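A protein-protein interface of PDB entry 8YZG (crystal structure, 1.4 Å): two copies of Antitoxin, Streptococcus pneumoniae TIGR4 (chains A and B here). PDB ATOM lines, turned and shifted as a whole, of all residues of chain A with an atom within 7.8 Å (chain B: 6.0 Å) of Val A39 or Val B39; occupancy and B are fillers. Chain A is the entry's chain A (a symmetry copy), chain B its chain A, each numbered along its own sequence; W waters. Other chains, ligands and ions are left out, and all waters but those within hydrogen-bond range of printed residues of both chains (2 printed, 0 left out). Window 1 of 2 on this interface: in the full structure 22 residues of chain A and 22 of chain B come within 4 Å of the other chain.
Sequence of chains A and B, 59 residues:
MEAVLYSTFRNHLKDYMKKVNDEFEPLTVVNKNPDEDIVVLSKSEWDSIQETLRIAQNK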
ATOM      1  N   MET A   1     -10.729 -11.716 -27.084  1.00  0.00           N
ATOM      2  CA  MET A   1      -9.933 -10.573 -26.650  1.00  0.00           C
ATOM      3  C   MET A   1      -8.841 -10.241 -27.663  1.00  0.00           C
ATOM      4  O   MET A   1      -8.233 -11.149 -28.229  1.00  0.00           O
ATOM      5  CB  MET A   1      -9.294 -10.863 -25.288  1.00  0.00           C
ATOM      6  CG  MET A   1      -8.633  -9.643 -24.682  1.00  0.00           C
ATOM      7  SD  MET A   1      -7.730  -9.907 -23.154  1.00  0.00           S
ATOM      8  CE  MET A   1      -8.880 -10.862 -22.181  1.00  0.00           C
ATOM      9  N   GLU A   2      -8.591  -8.948 -27.880  1.00  0.00           N
ATOM     10  CA  GLU A   2      -7.503  -8.544 -28.764  1.00  0.00           C
ATOM     11  C   GLU A   2      -6.180  -9.083 -28.236  1.00  0.00           C
ATOM     12  O   GLU A   2      -5.904  -9.049 -27.032  1.00  0.00           O
ATOM     13  CB  GLU A   2      -7.439  -7.013 -28.906  1.00  0.00           C
ATOM     14  CG  GLU A   2      -6.382  -6.486 -29.914  1.00  0.00           C
ATOM     15  CD  GLU A   2      -6.653  -5.053 -30.406  1.00  0.00           C
ATOM     16  OE1 GLU A   2      -7.703  -4.490 -30.031  1.00  0.00           O
ATOM     17  OE2 GLU A   2      -5.823  -4.484 -31.165  1.00  0.00           O
ATOM     18  N   PHE A   9       3.347  -4.298 -28.974  1.00  0.00           N
ATOM     19  CA  PHE A   9       2.935  -3.610 -27.755  1.00  0.00           C
ATOM     20  C   PHE A   9       4.007  -2.623 -27.287  1.00  0.00           C
ATOM     21  O   PHE A   9       3.716  -1.449 -27.028  1.00  0.00           O
ATOM     22  CB  PHE A   9       2.638  -4.674 -26.696  1.00  0.00           C
ATOM     23  CG  PHE A   9       2.194  -4.117 -25.375  1.00  0.00           C
ATOM     24  CD1 PHE A   9       0.965  -3.493 -25.241  1.00  0.00           C
ATOM     25  CD2 PHE A   9       3.014  -4.212 -24.262  1.00  0.00           C
ATOM     26  CE1 PHE A   9       0.552  -2.970 -24.008  1.00  0.00           C
ATOM     27  CE2 PHE A   9       2.598  -3.710 -23.029  1.00  0.00           C
ATOM     28  CZ  PHE A   9       1.382  -3.083 -22.910  1.00  0.00           C
ATOM     29  N   VAL A  20      -7.088   0.745 -24.387  1.00  0.00           N
ATOM     30  CA  VAL A  20      -7.830   0.007 -23.368  1.00  0.00           C
ATOM     31  C   VAL A  20      -8.671   0.954 -22.543  1.00  0.00           C
ATOM     32  O   VAL A  20      -9.761   0.587 -22.083  1.00  0.00           O
ATOM     33  CB  VAL A  20      -6.934  -0.904 -22.506  1.00  0.00           C
ATOM     34  CG1 VAL A  20      -6.201  -1.914 -23.387  1.00  0.00           C
ATOM     35  CG2 VAL A  20      -5.963  -0.099 -21.660  1.00  0.00           C
ATOM     36  N   ASN A  21      -8.196   2.187 -22.353  1.00  0.00           N
ATOM     37  CA  ASN A  21      -8.996   3.199 -21.668  1.00  0.00           C
ATOM     38  C   ASN A  21     -10.189   3.622 -22.510  1.00  0.00           C
ATOM     39  O   ASN A  21     -11.331   3.622 -22.037  1.00  0.00           O
ATOM     40  CB  ASN A  21      -8.112   4.402 -21.344  1.00  0.00           C
ATOM     41  CG  ASN A  21      -7.420   4.256 -20.020  1.00  0.00           C
ATOM     42  OD1 ASN A  21      -7.997   4.522 -18.974  1.00  0.00           O
ATOM     43  ND2 ASN A  21      -6.171   3.804 -20.052  1.00  0.00           N
ATOM     44  N   GLU A  25     -11.993  -2.155 -22.909  1.00  0.00           N
ATOM     45  CA  GLU A  25     -11.765  -3.536 -23.352  1.00  0.00           C
ATOM     46  C   GLU A  25     -10.309  -3.908 -23.073  1.00  0.00           C
ATOM     47  O   GLU A  25      -9.397  -3.145 -23.448  1.00  0.00           O
ATOM     48  CB  GLU A  25     -12.056  -3.721 -24.848  1.00  0.00           C
ATOM     49  CG  GLU A  25     -13.510  -3.558 -25.253  1.00  0.00           C
ATOM     50  CD  GLU A  25     -14.328  -4.796 -24.977  1.00  0.00           C
ATOM     51  OE1 GLU A  25     -13.764  -5.802 -24.493  1.00  0.00           O
ATOM     52  OE2 GLU A  25     -15.552  -4.760 -25.245  1.00  0.00           O
ATOM     53  N   PRO A  26     -10.068  -5.051 -22.441  1.00  0.00           N
ATOM     54  CA  PRO A  26      -8.694  -5.508 -22.177  1.00  0.00           C
ATOM     55  C   PRO A  26      -8.044  -6.047 -23.445  1.00  0.00           C
ATOM     56  O   PRO A  26      -8.701  -6.342 -24.443  1.00  0.00           O
ATOM     57  CB  PRO A  26      -8.912  -6.669 -21.209  1.00  0.00           C
ATOM     58  CG  PRO A  26     -10.241  -7.257 -21.676  1.00  0.00           C
ATOM     59  CD  PRO A  26     -11.078  -6.052 -22.053  1.00  0.00           C
ATOM     60  N   LEU A  27      -6.726  -6.209 -23.379  1.00  0.00           N
ATOM     61  CA  LEU A  27      -6.013  -6.911 -24.433  1.00  0.00           C
ATOM     62  C   LEU A  27      -4.995  -7.839 -23.795  1.00  0.00           C
ATOM     63  O   LEU A  27      -4.594  -7.652 -22.647  1.00  0.00           O
ATOM     64  CB  LEU A  27      -5.356  -5.945 -25.429  1.00  0.00           C
ATOM     65  CG  LEU A  27      -4.287  -4.993 -24.893  1.00  0.00           C
ATOM     66  CD1 LEU A  27      -2.888  -5.606 -24.766  1.00  0.00           C
ATOM     67  CD2 LEU A  27      -4.252  -3.778 -25.814  1.00  0.00           C
ATOM     68  N   THR A  28      -4.568  -8.846 -24.548  1.00  0.00           N
ATOM     69  CA  THR A  28      -3.536  -9.778 -24.114  1.00  0.00           C
ATOM     70  C   THR A  28      -2.268  -9.491 -24.897  1.00  0.00           C
ATOM     71  O   THR A  28      -2.321  -9.273 -26.110  1.00  0.00           O
ATOM     72  CB  THR A  28      -3.942 -11.236 -24.357  1.00  0.00           C
ATOM     73  OG1 THR A  28      -4.205 -11.470 -25.740  1.00  0.00           O
ATOM     74  CG2 THR A  28      -5.125 -11.643 -23.541  1.00  0.00           C
ATOM     75  N   VAL A  29      -1.134  -9.466 -24.203  1.00  0.00           N
ATOM     76  CA  VAL A  29       0.174  -9.355 -24.841  1.00  0.00           C
ATOM     77  C   VAL A  29       0.797 -10.738 -24.925  1.00  0.00           C
ATOM     78  O   VAL A  29       0.916 -11.447 -23.909  1.00  0.00           O
ATOM     79  CB  VAL A  29       1.080  -8.358 -24.111  1.00  0.00           C
ATOM     80  CG1 VAL A  29       2.404  -8.218 -24.855  1.00  0.00           C
ATOM     81  CG2 VAL A  29       0.379  -7.013 -23.990  1.00  0.00           C
ATOM     82  N   VAL A  30       1.181 -11.108 -26.146  1.00  0.00           N
ATOM     83  CA  VAL A  30       1.611 -12.453 -26.513  1.00  0.00           C
ATOM     84  C   VAL A  30       3.135 -12.469 -26.532  1.00  0.00           C
ATOM     85  O   VAL A  30       3.761 -11.717 -27.283  1.00  0.00           O
ATOM     86  CB  VAL A  30       1.043 -12.832 -27.894  1.00  0.00           C
ATOM     87  CG1 VAL A  30       1.548 -14.178 -28.340  1.00  0.00           C
ATOM     88  CG2 VAL A  30      -0.485 -12.793 -27.893  1.00  0.00           C
ATOM     89  N   GLU A  36       5.542 -15.024 -19.652  1.00  0.00           N
ATOM     90  CA  GLU A  36       5.658 -13.577 -19.674  1.00  0.00           C
ATOM     91  C   GLU A  36       4.358 -12.922 -20.108  1.00  0.00           C
ATOM     92  O   GLU A  36       4.257 -11.686 -20.122  1.00  0.00           O
ATOM     93  CB  GLU A  36       6.794 -13.146 -20.611  1.00  0.00           C
ATOM     94  CG  GLU A  36       8.202 -13.431 -20.090  1.00  0.00           C
ATOM     95  CD  GLU A  36       9.245 -13.274 -21.184  1.00  0.00           C
ATOM     96  OE1 GLU A  36       8.872 -12.827 -22.295  1.00  0.00           O
ATOM     97  OE2 GLU A  36      10.424 -13.597 -20.933  1.00  0.00           O
ATOM     98  N   ASP A  37       3.354 -13.715 -20.431  1.00  0.00           N
ATOM     99  CA  ASP A  37       2.162 -13.171 -21.074  1.00  0.00           C
ATOM    100  C   ASP A  37       1.296 -12.439 -20.074  1.00  0.00           C
ATOM    101  O   ASP A  37       1.182 -12.829 -18.908  1.00  0.00           O
ATOM    102  CB  ASP A  37       1.346 -14.266 -21.753  1.00  0.00           C
ATOM    103  CG  ASP A  37       1.899 -14.641 -23.122  1.00  0.00           C
ATOM    104  OD1 ASP A  37       3.080 -14.389 -23.361  1.00  0.00           O
ATOM    105  OD2 ASP A  37       1.132 -15.134 -23.962  1.00  0.00           O
ATOM    106  N   ILE A  38       0.676 -11.367 -20.536  1.00  0.00           N
ATOM    107  CA  ILE A  38      -0.024 -10.462 -19.644  1.00  0.00           C
ATOM    108  C   ILE A  38      -1.338 -10.038 -20.264  1.00  0.00           C
ATOM    109  O   ILE A  38      -1.590 -10.207 -21.462  1.00  0.00           O
ATOM    110  CB  ILE A  38       0.795  -9.211 -19.247  1.00  0.00           C
ATOM    111  CG1 ILE A  38       1.167  -8.385 -20.477  1.00  0.00           C
ATOM    112  CG2 ILE A  38       2.038  -9.587 -18.452  1.00  0.00           C
ATOM    113  CD1 ILE A  38       1.604  -6.969 -20.152  1.00  0.00           C
ATOM    114  N   VAL A  39      -2.181  -9.494 -19.407  1.00  0.00           N
ATOM    115  CA  VAL A  39      -3.399  -8.805 -19.776  1.00  0.00           C
ATOM    116  C   VAL A  39      -3.258  -7.364 -19.305  1.00  0.00           C
ATOM    117  O   VAL A  39      -2.725  -7.098 -18.215  1.00  0.00           O
ATOM    118  CB  VAL A  39      -4.647  -9.498 -19.190  1.00  0.00           C
ATOM    119  CG1 VAL A  39      -5.878  -8.621 -19.361  1.00  0.00           C
ATOM    120  CG2 VAL A  39      -4.850 -10.858 -19.859  1.00  0.00           C
ATOM    121  N   VAL A  40      -3.680  -6.446 -20.169  1.00  0.00           N
ATOM    122  CA  VAL A  40      -3.623  -5.015 -19.933  1.00  0.00           C
ATOM    123  C   VAL A  40      -5.048  -4.494 -20.038  1.00  0.00           C
ATOM    124  O   VAL A  40      -5.762  -4.813 -20.996  1.00  0.00           O
ATOM    125  CB  VAL A  40      -2.733  -4.339 -20.995  1.00  0.00           C
ATOM    126  CG1 VAL A  40      -2.731  -2.826 -20.822  1.00  0.00           C
ATOM    127  CG2 VAL A  40      -1.304  -4.898 -20.972  1.00  0.00           C
ATOM    128  N   LEU A  41      -5.467  -3.698 -19.062  1.00  0.00           N
ATOM    129  CA  LEU A  41      -6.795  -3.101 -19.088  1.00  0.00           C
ATOM    130  C   LEU A  41      -6.738  -1.758 -18.381  1.00  0.00           C
ATOM    131  O   LEU A  41      -5.768  -1.439 -17.686  1.00  0.00           O
ATOM    132  CB  LEU A  41      -7.880  -4.015 -18.486  1.00  0.00           C
ATOM    133  CG  LEU A  41      -7.887  -4.277 -16.988  1.00  0.00           C
ATOM    134  CD1 LEU A  41      -9.240  -4.846 -16.579  1.00  0.00           C
ATOM    135  CD2 LEU A  41      -6.768  -5.236 -16.582  1.00  0.00           C
ATOM    136  N   SER A  42      -7.770  -0.944 -18.567  1.00  0.00           N
ATOM    137  CA  SER A  42      -7.767   0.336 -17.875  1.00  0.00           C
ATOM    138  C   SER A  42      -7.977   0.149 -16.374  1.00  0.00           C
ATOM    139  O   SER A  42      -8.613  -0.813 -15.917  1.00  0.00           O
ATOM    140  CB  SER A  42      -8.826   1.271 -18.457  1.00  0.00           C
ATOM    141  OG  SER A  42     -10.138   0.819 -18.168  1.00  0.00           O
ATOM    142  N   LYS A  43      -7.422   1.082 -15.593  1.00  0.00           N
ATOM    143  CA  LYS A  43      -7.744   1.111 -14.172  1.00  0.00           C
ATOM    144  C   LYS A  43      -9.246   1.244 -13.959  1.00  0.00           C
ATOM    145  O   LYS A  43      -9.806   0.617 -13.058  1.00  0.00           O
ATOM    146  CB  LYS A  43      -6.986   2.251 -13.491  1.00  0.00           C
ATOM    147  CG  LYS A  43      -7.174   2.327 -11.975  1.00  0.00           C
ATOM    148  CD  LYS A  43      -6.705   1.057 -11.291  1.00  0.00           C
ATOM    149  CE  LYS A  43      -6.486   1.272  -9.797  1.00  0.00           C
ATOM    150  NZ  LYS A  43      -7.632   1.978  -9.164  1.00  0.00           N
ATOM    151  N   SER A  44      -9.920   2.023 -14.806  1.00  0.00           N
ATOM    152  CA  SER A  44     -11.372   2.151 -14.687  1.00  0.00           C
ATOM    153  C   SER A  44     -12.064   0.797 -14.809  1.00  0.00           C
ATOM    154  O   SER A  44     -12.937   0.453 -14.001  1.00  0.00           O
ATOM    155  CB  SER A  44     -11.867   3.117 -15.760  1.00  0.00           C
ATOM    156  OG  SER A  44     -13.274   3.267 -15.731  1.00  0.00           O
ATOM    157  N   GLU A  45     -11.701   0.006 -15.823  1.00  0.00           N
ATOM    158  CA  GLU A  45     -12.319  -1.303 -15.971  1.00  0.00           C
ATOM    159  C   GLU A  45     -11.925  -2.249 -14.842  1.00  0.00           C
ATOM    160  O   GLU A  45     -12.759  -3.032 -14.361  1.00  0.00           O
ATOM    161  CB  GLU A  45     -12.011  -1.919 -17.334  1.00  0.00           C
ATOM    162  CG  GLU A  45     -12.797  -3.192 -17.555  1.00  0.00           C
ATOM    163  CD  GLU A  45     -12.596  -3.842 -18.903  1.00  0.00           C
ATOM    164  OE1 GLU A  45     -11.780  -3.369 -19.728  1.00  0.00           O
ATOM    165  OE2 GLU A  45     -13.277  -4.865 -19.146  1.00  0.00           O
ATOM    166  N   TRP A  46     -10.659  -2.219 -14.412  1.00  0.00           N
ATOM    167  CA  TRP A  46     -10.269  -3.053 -13.276  1.00  0.00           C
ATOM    168  C   TRP A  46     -11.094  -2.710 -12.043  1.00  0.00           C
ATOM    169  O   TRP A  46     -11.570  -3.606 -11.327  1.00  0.00           O
ATOM    170  CB  TRP A  46      -8.782  -2.870 -12.989  1.00  0.00           C
ATOM    171  CG  TRP A  46      -8.316  -3.554 -11.754  1.00  0.00           C
ATOM    172  CD1 TRP A  46      -8.155  -3.002 -10.512  1.00  0.00           C
ATOM    173  CD2 TRP A  46      -7.944  -4.929 -11.640  1.00  0.00           C
ATOM    174  NE1 TRP A  46      -7.711  -3.960  -9.627  1.00  0.00           N
ATOM    175  CE2 TRP A  46      -7.562  -5.147 -10.294  1.00  0.00           C
ATOM    176  CE3 TRP A  46      -7.891  -5.998 -12.540  1.00  0.00           C
ATOM    177  CZ2 TRP A  46      -7.135  -6.396  -9.834  1.00  0.00           C
ATOM    178  CZ3 TRP A  46      -7.472  -7.241 -12.074  1.00  0.00           C
ATOM    179  CH2 TRP A  46      -7.096  -7.423 -10.737  1.00  0.00           C
ATOM    180  N   ASP A  47     -11.253  -1.411 -11.772  1.00  0.00           N
ATOM    181  CA  ASP A  47     -12.032  -0.980 -10.613  1.00  0.00           C
ATOM    182  C   ASP A  47     -13.475  -1.422 -10.747  1.00  0.00           C
ATOM    183  O   ASP A  47     -14.084  -1.858  -9.764  1.00  0.00           O
ATOM    184  CB  ASP A  47     -11.989   0.540 -10.476  1.00  0.00           C
ATOM    185  CG  ASP A  47     -10.657   1.048  -9.999  1.00  0.00           C
ATOM    186  OD1 ASP A  47      -9.836   0.232  -9.539  1.00  0.00           O
ATOM    187  OD2 ASP A  47     -10.429   2.274 -10.108  1.00  0.00           O
ATOM    188  N   GLN A  50     -13.547  -4.990  -9.743  1.00  0.00           N
ATOM    189  CA  GLN A  50     -13.358  -5.203  -8.309  1.00  0.00           C
ATOM    190  C   GLN A  50     -14.551  -4.702  -7.500  1.00  0.00           C
ATOM    191  O   GLN A  50     -14.957  -5.342  -6.520  1.00  0.00           O
ATOM    192  CB  GLN A  50     -12.060  -4.552  -7.842  1.00  0.00           C
ATOM    193  CG  GLN A  50     -10.786  -5.174  -8.444  1.00  0.00           C
ATOM    194  CD  GLN A  50     -10.646  -6.667  -8.174  1.00  0.00           C
ATOM    195  OE1 GLN A  50     -10.993  -7.149  -7.098  1.00  0.00           O
ATOM    196  NE2 GLN A  50     -10.122  -7.401  -9.149  1.00  0.00           N
ATOM    197  N   MET B   1      -2.106  -2.287  -4.091  1.00  0.00           N
ATOM    198  CA  MET B   1      -1.495  -2.758  -5.329  1.00  0.00           C
ATOM    199  C   MET B   1      -0.232  -1.967  -5.659  1.00  0.00           C
ATOM    200  O   MET B   1      -0.199  -0.753  -5.459  1.00  0.00           O
ATOM    201  CB  MET B   1      -2.489  -2.638  -6.488  1.00  0.00           C
ATOM    202  CG  MET B   1      -1.995  -3.307  -7.752  1.00  0.00           C
ATOM    203  SD  MET B   1      -3.020  -3.101  -9.211  1.00  0.00           S
ATOM    204  CE  MET B   1      -4.652  -3.473  -8.597  1.00  0.00           C
ATOM    205  N   PRO B  26      -1.235  -8.221  -9.608  1.00  0.00           N
ATOM    206  CA  PRO B  26      -1.314  -7.147 -10.611  1.00  0.00           C
ATOM    207  C   PRO B  26      -0.526  -5.922 -10.164  1.00  0.00           C
ATOM    208  O   PRO B  26      -0.163  -5.767  -8.998  1.00  0.00           O
ATOM    209  CB  PRO B  26      -2.801  -6.799 -10.606  1.00  0.00           C
ATOM    210  CG  PRO B  26      -3.202  -7.035  -9.153  1.00  0.00           C
ATOM    211  CD  PRO B  26      -2.425  -8.269  -8.741  1.00  0.00           C
ATOM    212  N   LEU B  27      -0.295  -5.021 -11.114  1.00  0.00           N
ATOM    213  CA  LEU B  27       0.254  -3.717 -10.779  1.00  0.00           C
ATOM    214  C   LEU B  27      -0.491  -2.659 -11.572  1.00  0.00           C
ATOM    215  O   LEU B  27      -1.105  -2.947 -12.600  1.00  0.00           O
ATOM    216  CB  LEU B  27       1.769  -3.648 -11.022  1.00  0.00           C
ATOM    217  CG  LEU B  27       2.267  -3.853 -12.453  1.00  0.00           C
ATOM    218  CD1 LEU B  27       2.200  -2.605 -13.339  1.00  0.00           C
ATOM    219  CD2 LEU B  27       3.700  -4.368 -12.369  1.00  0.00           C
ATOM    220  N   THR B  28      -0.433  -1.422 -11.096  1.00  0.00           N
ATOM    221  CA  THR B  28      -1.028  -0.280 -11.780  1.00  0.00           C
ATOM    222  C   THR B  28       0.089   0.570 -12.358  1.00  0.00           C
ATOM    223  O   THR B  28       1.099   0.808 -11.690  1.00  0.00           O
ATOM    224  CB  THR B  28      -1.861   0.586 -10.830  1.00  0.00           C
ATOM    225  OG1 THR B  28      -1.064   1.074  -9.752  1.00  0.00           O
ATOM    226  CG2 THR B  28      -3.051  -0.138 -10.293  1.00  0.00           C
ATOM    227  N   VAL B  29      -0.078   1.005 -13.603  1.00  0.00           N
ATOM    228  CA  VAL B  29       0.835   1.953 -14.233  1.00  0.00           C
ATOM    229  C   VAL B  29       0.226   3.343 -14.157  1.00  0.00           C
ATOM    230  O   VAL B  29      -0.921   3.562 -14.586  1.00  0.00           O
ATOM    231  CB  VAL B  29       1.171   1.548 -15.672  1.00  0.00           C
ATOM    232  CG1 VAL B  29       2.186   2.523 -16.261  1.00  0.00           C
ATOM    233  CG2 VAL B  29       1.706   0.125 -15.698  1.00  0.00           C
ATOM    234  N   ASP B  37      -4.168   5.445 -17.603  1.00  0.00           N
ATOM    235  CA  ASP B  37      -3.704   4.553 -16.544  1.00  0.00           C
ATOM    236  C   ASP B  37      -4.238   3.153 -16.745  1.00  0.00           C
ATOM    237  O   ASP B  37      -5.368   2.950 -17.202  1.00  0.00           O
ATOM    238  CB  ASP B  37      -4.113   5.064 -15.167  1.00  0.00           C
ATOM    239  CG  ASP B  37      -3.177   6.148 -14.647  1.00  0.00           C
ATOM    240  OD1 ASP B  37      -2.507   6.779 -15.464  1.00  0.00           O
ATOM    241  OD2 ASP B  37      -3.083   6.320 -13.422  1.00  0.00           O
ATOM    242  N   ILE B  38      -3.419   2.177 -16.397  1.00  0.00           N
ATOM    243  CA  ILE B  38      -3.721   0.794 -16.717  1.00  0.00           C
ATOM    244  C   ILE B  38      -3.383  -0.096 -15.540  1.00  0.00           C
ATOM    245  O   ILE B  38      -2.679   0.289 -14.600  1.00  0.00           O
ATOM    246  CB  ILE B  38      -3.009   0.273 -17.989  1.00  0.00           C
ATOM    247  CG1 ILE B  38      -1.490   0.348 -17.836  1.00  0.00           C
ATOM    248  CG2 ILE B  38      -3.465   1.024 -19.232  1.00  0.00           C
ATOM    249  CD1 ILE B  38      -0.734  -0.499 -18.843  1.00  0.00           C
ATOM    250  N   VAL B  39      -3.922  -1.299 -15.609  1.00  0.00           N
ATOM    251  CA  VAL B  39      -3.578  -2.404 -14.742  1.00  0.00           C
ATOM    252  C   VAL B  39      -2.999  -3.502 -15.623  1.00  0.00           C
ATOM    253  O   VAL B  39      -3.483  -3.745 -16.742  1.00  0.00           O
ATOM    254  CB  VAL B  39      -4.794  -2.886 -13.921  1.00  0.00           C
ATOM    255  CG1 VAL B  39      -4.484  -4.202 -13.225  1.00  0.00           C
ATOM    256  CG2 VAL B  39      -5.196  -1.815 -12.908  1.00  0.00           C
ATOM    257  N   VAL B  40      -1.922  -4.108 -15.133  1.00  0.00           N
ATOM    258  CA  VAL B  40      -1.200  -5.167 -15.813  1.00  0.00           C
ATOM    259  C   VAL B  40      -1.213  -6.374 -14.887  1.00  0.00           C
ATOM    260  O   VAL B  40      -0.911  -6.251 -13.695  1.00  0.00           O
ATOM    261  CB  VAL B  40       0.252  -4.726 -16.087  1.00  0.00           C
ATOM    262  CG1 VAL B  40       1.054  -5.856 -16.719  1.00  0.00           C
ATOM    263  CG2 VAL B  40       0.303  -3.462 -16.955  1.00  0.00           C
ATOM    264  N   LEU B  41      -1.563  -7.536 -15.425  1.00  0.00           N
ATOM    265  CA  LEU B  41      -1.559  -8.765 -14.644  1.00  0.00           C
ATOM    266  C   LEU B  41      -1.237  -9.927 -15.567  1.00  0.00           C
ATOM    267  O   LEU B  41      -1.273  -9.801 -16.795  1.00  0.00           O
ATOM    268  CB  LEU B  41      -2.875  -8.995 -13.876  1.00  0.00           C
ATOM    269  CG  LEU B  41      -4.139  -9.340 -14.649  1.00  0.00           C
ATOM    270  CD1 LEU B  41      -5.179  -9.912 -13.693  1.00  0.00           C
ATOM    271  CD2 LEU B  41      -4.704  -8.116 -15.371  1.00  0.00           C
ATOM    272  N   SER B  42      -0.898 -11.071 -14.985  1.00  0.00           N
ATOM    273  CA  SER B  42      -0.620 -12.218 -15.838  1.00  0.00           C
ATOM    274  C   SER B  42      -1.898 -12.740 -16.490  1.00  0.00           C
ATOM    275  O   SER B  42      -3.008 -12.610 -15.951  1.00  0.00           O
ATOM    276  CB  SER B  42       0.077 -13.326 -15.050  1.00  0.00           C
ATOM    277  OG  SER B  42      -0.791 -13.912 -14.094  1.00  0.00           O
ATOM    278  N   LYS B  43      -1.739 -13.333 -17.679  1.00  0.00           N
ATOM    279  CA  LYS B  43      -2.858 -14.049 -18.277  1.00  0.00           C
ATOM    280  C   LYS B  43      -3.366 -15.139 -17.344  1.00  0.00           C
ATOM    281  O   LYS B  43      -4.574 -15.356 -17.236  1.00  0.00           O
ATOM    282  CB  LYS B  43      -2.441 -14.628 -19.629  1.00  0.00           C
ATOM    283  CG  LYS B  43      -3.562 -15.329 -20.398  1.00  0.00           C
ATOM    284  CD  LYS B  43      -4.710 -14.382 -20.695  1.00  0.00           C
ATOM    285  CE  LYS B  43      -5.612 -14.922 -21.799  1.00  0.00           C
ATOM    286  NZ  LYS B  43      -5.974 -16.348 -21.572  1.00  0.00           N
ATOM    287  N   TRP B  46      -5.567 -13.399 -14.829  1.00  0.00           N
ATOM    288  CA  TRP B  46      -6.801 -12.969 -15.483  1.00  0.00           C
ATOM    289  C   TRP B  46      -7.734 -14.150 -15.713  1.00  0.00           C
ATOM    290  O   TRP B  46      -8.947 -14.059 -15.466  1.00  0.00           O
ATOM    291  CB  TRP B  46      -6.471 -12.285 -16.806  1.00  0.00           C
ATOM    292  CG  TRP B  46      -7.664 -11.948 -17.626  1.00  0.00           C
ATOM    293  CD1 TRP B  46      -8.192 -12.675 -18.660  1.00  0.00           C
ATOM    294  CD2 TRP B  46      -8.486 -10.788 -17.485  1.00  0.00           C
ATOM    295  NE1 TRP B  46      -9.303 -12.034 -19.165  1.00  0.00           N
ATOM    296  CE2 TRP B  46      -9.499 -10.870 -18.471  1.00  0.00           C
ATOM    297  CE3 TRP B  46      -8.465  -9.683 -16.626  1.00  0.00           C
ATOM    298  CZ2 TRP B  46     -10.481  -9.885 -18.613  1.00  0.00           C
ATOM    299  CZ3 TRP B  46      -9.451  -8.710 -16.770  1.00  0.00           C
ATOM    300  CH2 TRP B  46     -10.436  -8.819 -17.758  1.00  0.00           C
HETATM  301  O   HOH W   1       0.233 -15.847 -17.755  1.00  0.00           O
HETATM  302  O   HOH W   2      -8.342   4.098 -16.117  1.00  0.00           O
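The backbone carbonyl oxygen (O) of Asp B37 lies within hydrogen-bond range of the side-chain amide nitrogen (ND2) of Asn A21 (3.1 Å). The backbone carbonyl oxygen (O) of Asp B37 lies within hydrogen-bond range of the backbone NH (N) of Lys A43, 3.2 Å away. The backbone carbonyl oxygen (O) of Leu A41 sits at hydrogen-bond distance from the backbone NH (N) of Val B39 (2.8 Å). The backbone NH (N) of Val A39 sits at hydrogen-bond distance from the backbone carbonyl oxygen (O) of Leu B41. The backbone NH (N) of Lys B43 lies within hydrogen-bond range of the backbone carbonyl oxygen (O) of Asp A37, at 3.2 Å.
The side-chain sulfur (SD) of Met B1 lies close to the backbone NH (N) of Thr B28. N of Val B29 sits at hydrogen-bond distance from O of Ile B38. The side-chain sulfur (SD) of Met A1 sits close to the backbone NH (N) of Thr A28, at 3.6 Å. The backbone carbonyl oxygen (O) of Leu A27 is in hydrogen-bond range of the backbone NH (N) of Val A40, at 2.9 Å. OG of Ser A42 sits at hydrogen-bond distance from N of Glu A45 (2.9 Å). NZ of Lys A43 is in salt-bridge range of OD1 of Asp A47, 2.8 Å away.
Ile B38 touches Val A20 (CG2 to CG2, 3.7 Å). Ile A38 touches Val B40. Lys B43 touches Ile A38 (N to CA, 3.9 Å). Val A39 touches Val B39. Val A39 touches Val B40. Trp B46 touches Val A39 (CB to CG2, 3.7 Å). O of Leu A41 touches CA of Ile B38, at 3.2 Å. Ile B38 touches Lys A43 (CA to N, 3.9 Å). CE of Met B1 touches NE1 of Trp A46 (3.3 Å). Trp A46 touches Leu B41 (CZ3 to CD1, 3.9 Å).
Glu A25 touches none of the printed residues of chain B. Of the printed residues of chain B, Thr A28 touches Lys B43 (3.7 Å). Printed residues of chain B within 4 Å of Ile A38: Val B40, Leu B41 and Lys B43. Val A39 touches just these residues of chain B: Val B39, Val B40, Leu B41, Lys B43 and Trp B46. Of the printed residues of chain B, Val A40 touches Ile B38 (3.6 Å) and Val B39 (3.4 Å). Val B29 touches none of the printed residues of chain A. The nearest residue of chain A that does not touch Val B39 is Ser A42 (4.4 Å).
Printed residues of chain B that touch a printed residue of chain A: Met B1, Thr B28, Asp B37, Ile B38, Val B39, Val B40, Leu B41, Ser B42, Lys B43 and Trp B46. Along chain B the printed residues that touch a printed residue of chain A span positions 1 to 46. Of the 24 printed residues of chain A, 12 touch a printed residue of chain B. Hydrophobic or aromatic side chains of chain A that line the printed part of chain B: Met A1, Val A20, Ile A38, Val A39, Val A40, Leu A41 and Trp A46. Among the printed residues, no Asp or Glu carboxylate lies within 4 Å of a Lys or Arg side-chain nitrogen of the other chain.
Thr A28 touches Lys B43, and with the chains exchanged Lys A43 touches Thr B28. Asp A37 touches Ser B42, and with the chains exchanged Ser A42 touches Asp B37. Ile A38 touches Val B40, and with the chains exchanged Val A40 touches Ile B38. Ile A38 touches Leu B41, and with the chains exchanged Leu A41 touches Ile B38. Positions printed for both chains: 1, 26, 27, 28, 29, 37, 38, 39, 40, 41, 42, 43 and 46. Of the 29 pairs that touch across the chains among the printed residues, 26 have their exchanged pair printed and touching as well.
Water W2 lies within hydrogen-bond range of OD1 of Asn A21, N of Ser A44, N of Lys A43 and O of Asp B37. Water W1 lies within hydrogen-bond range of N of Lys B43 and O of Asp A37.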
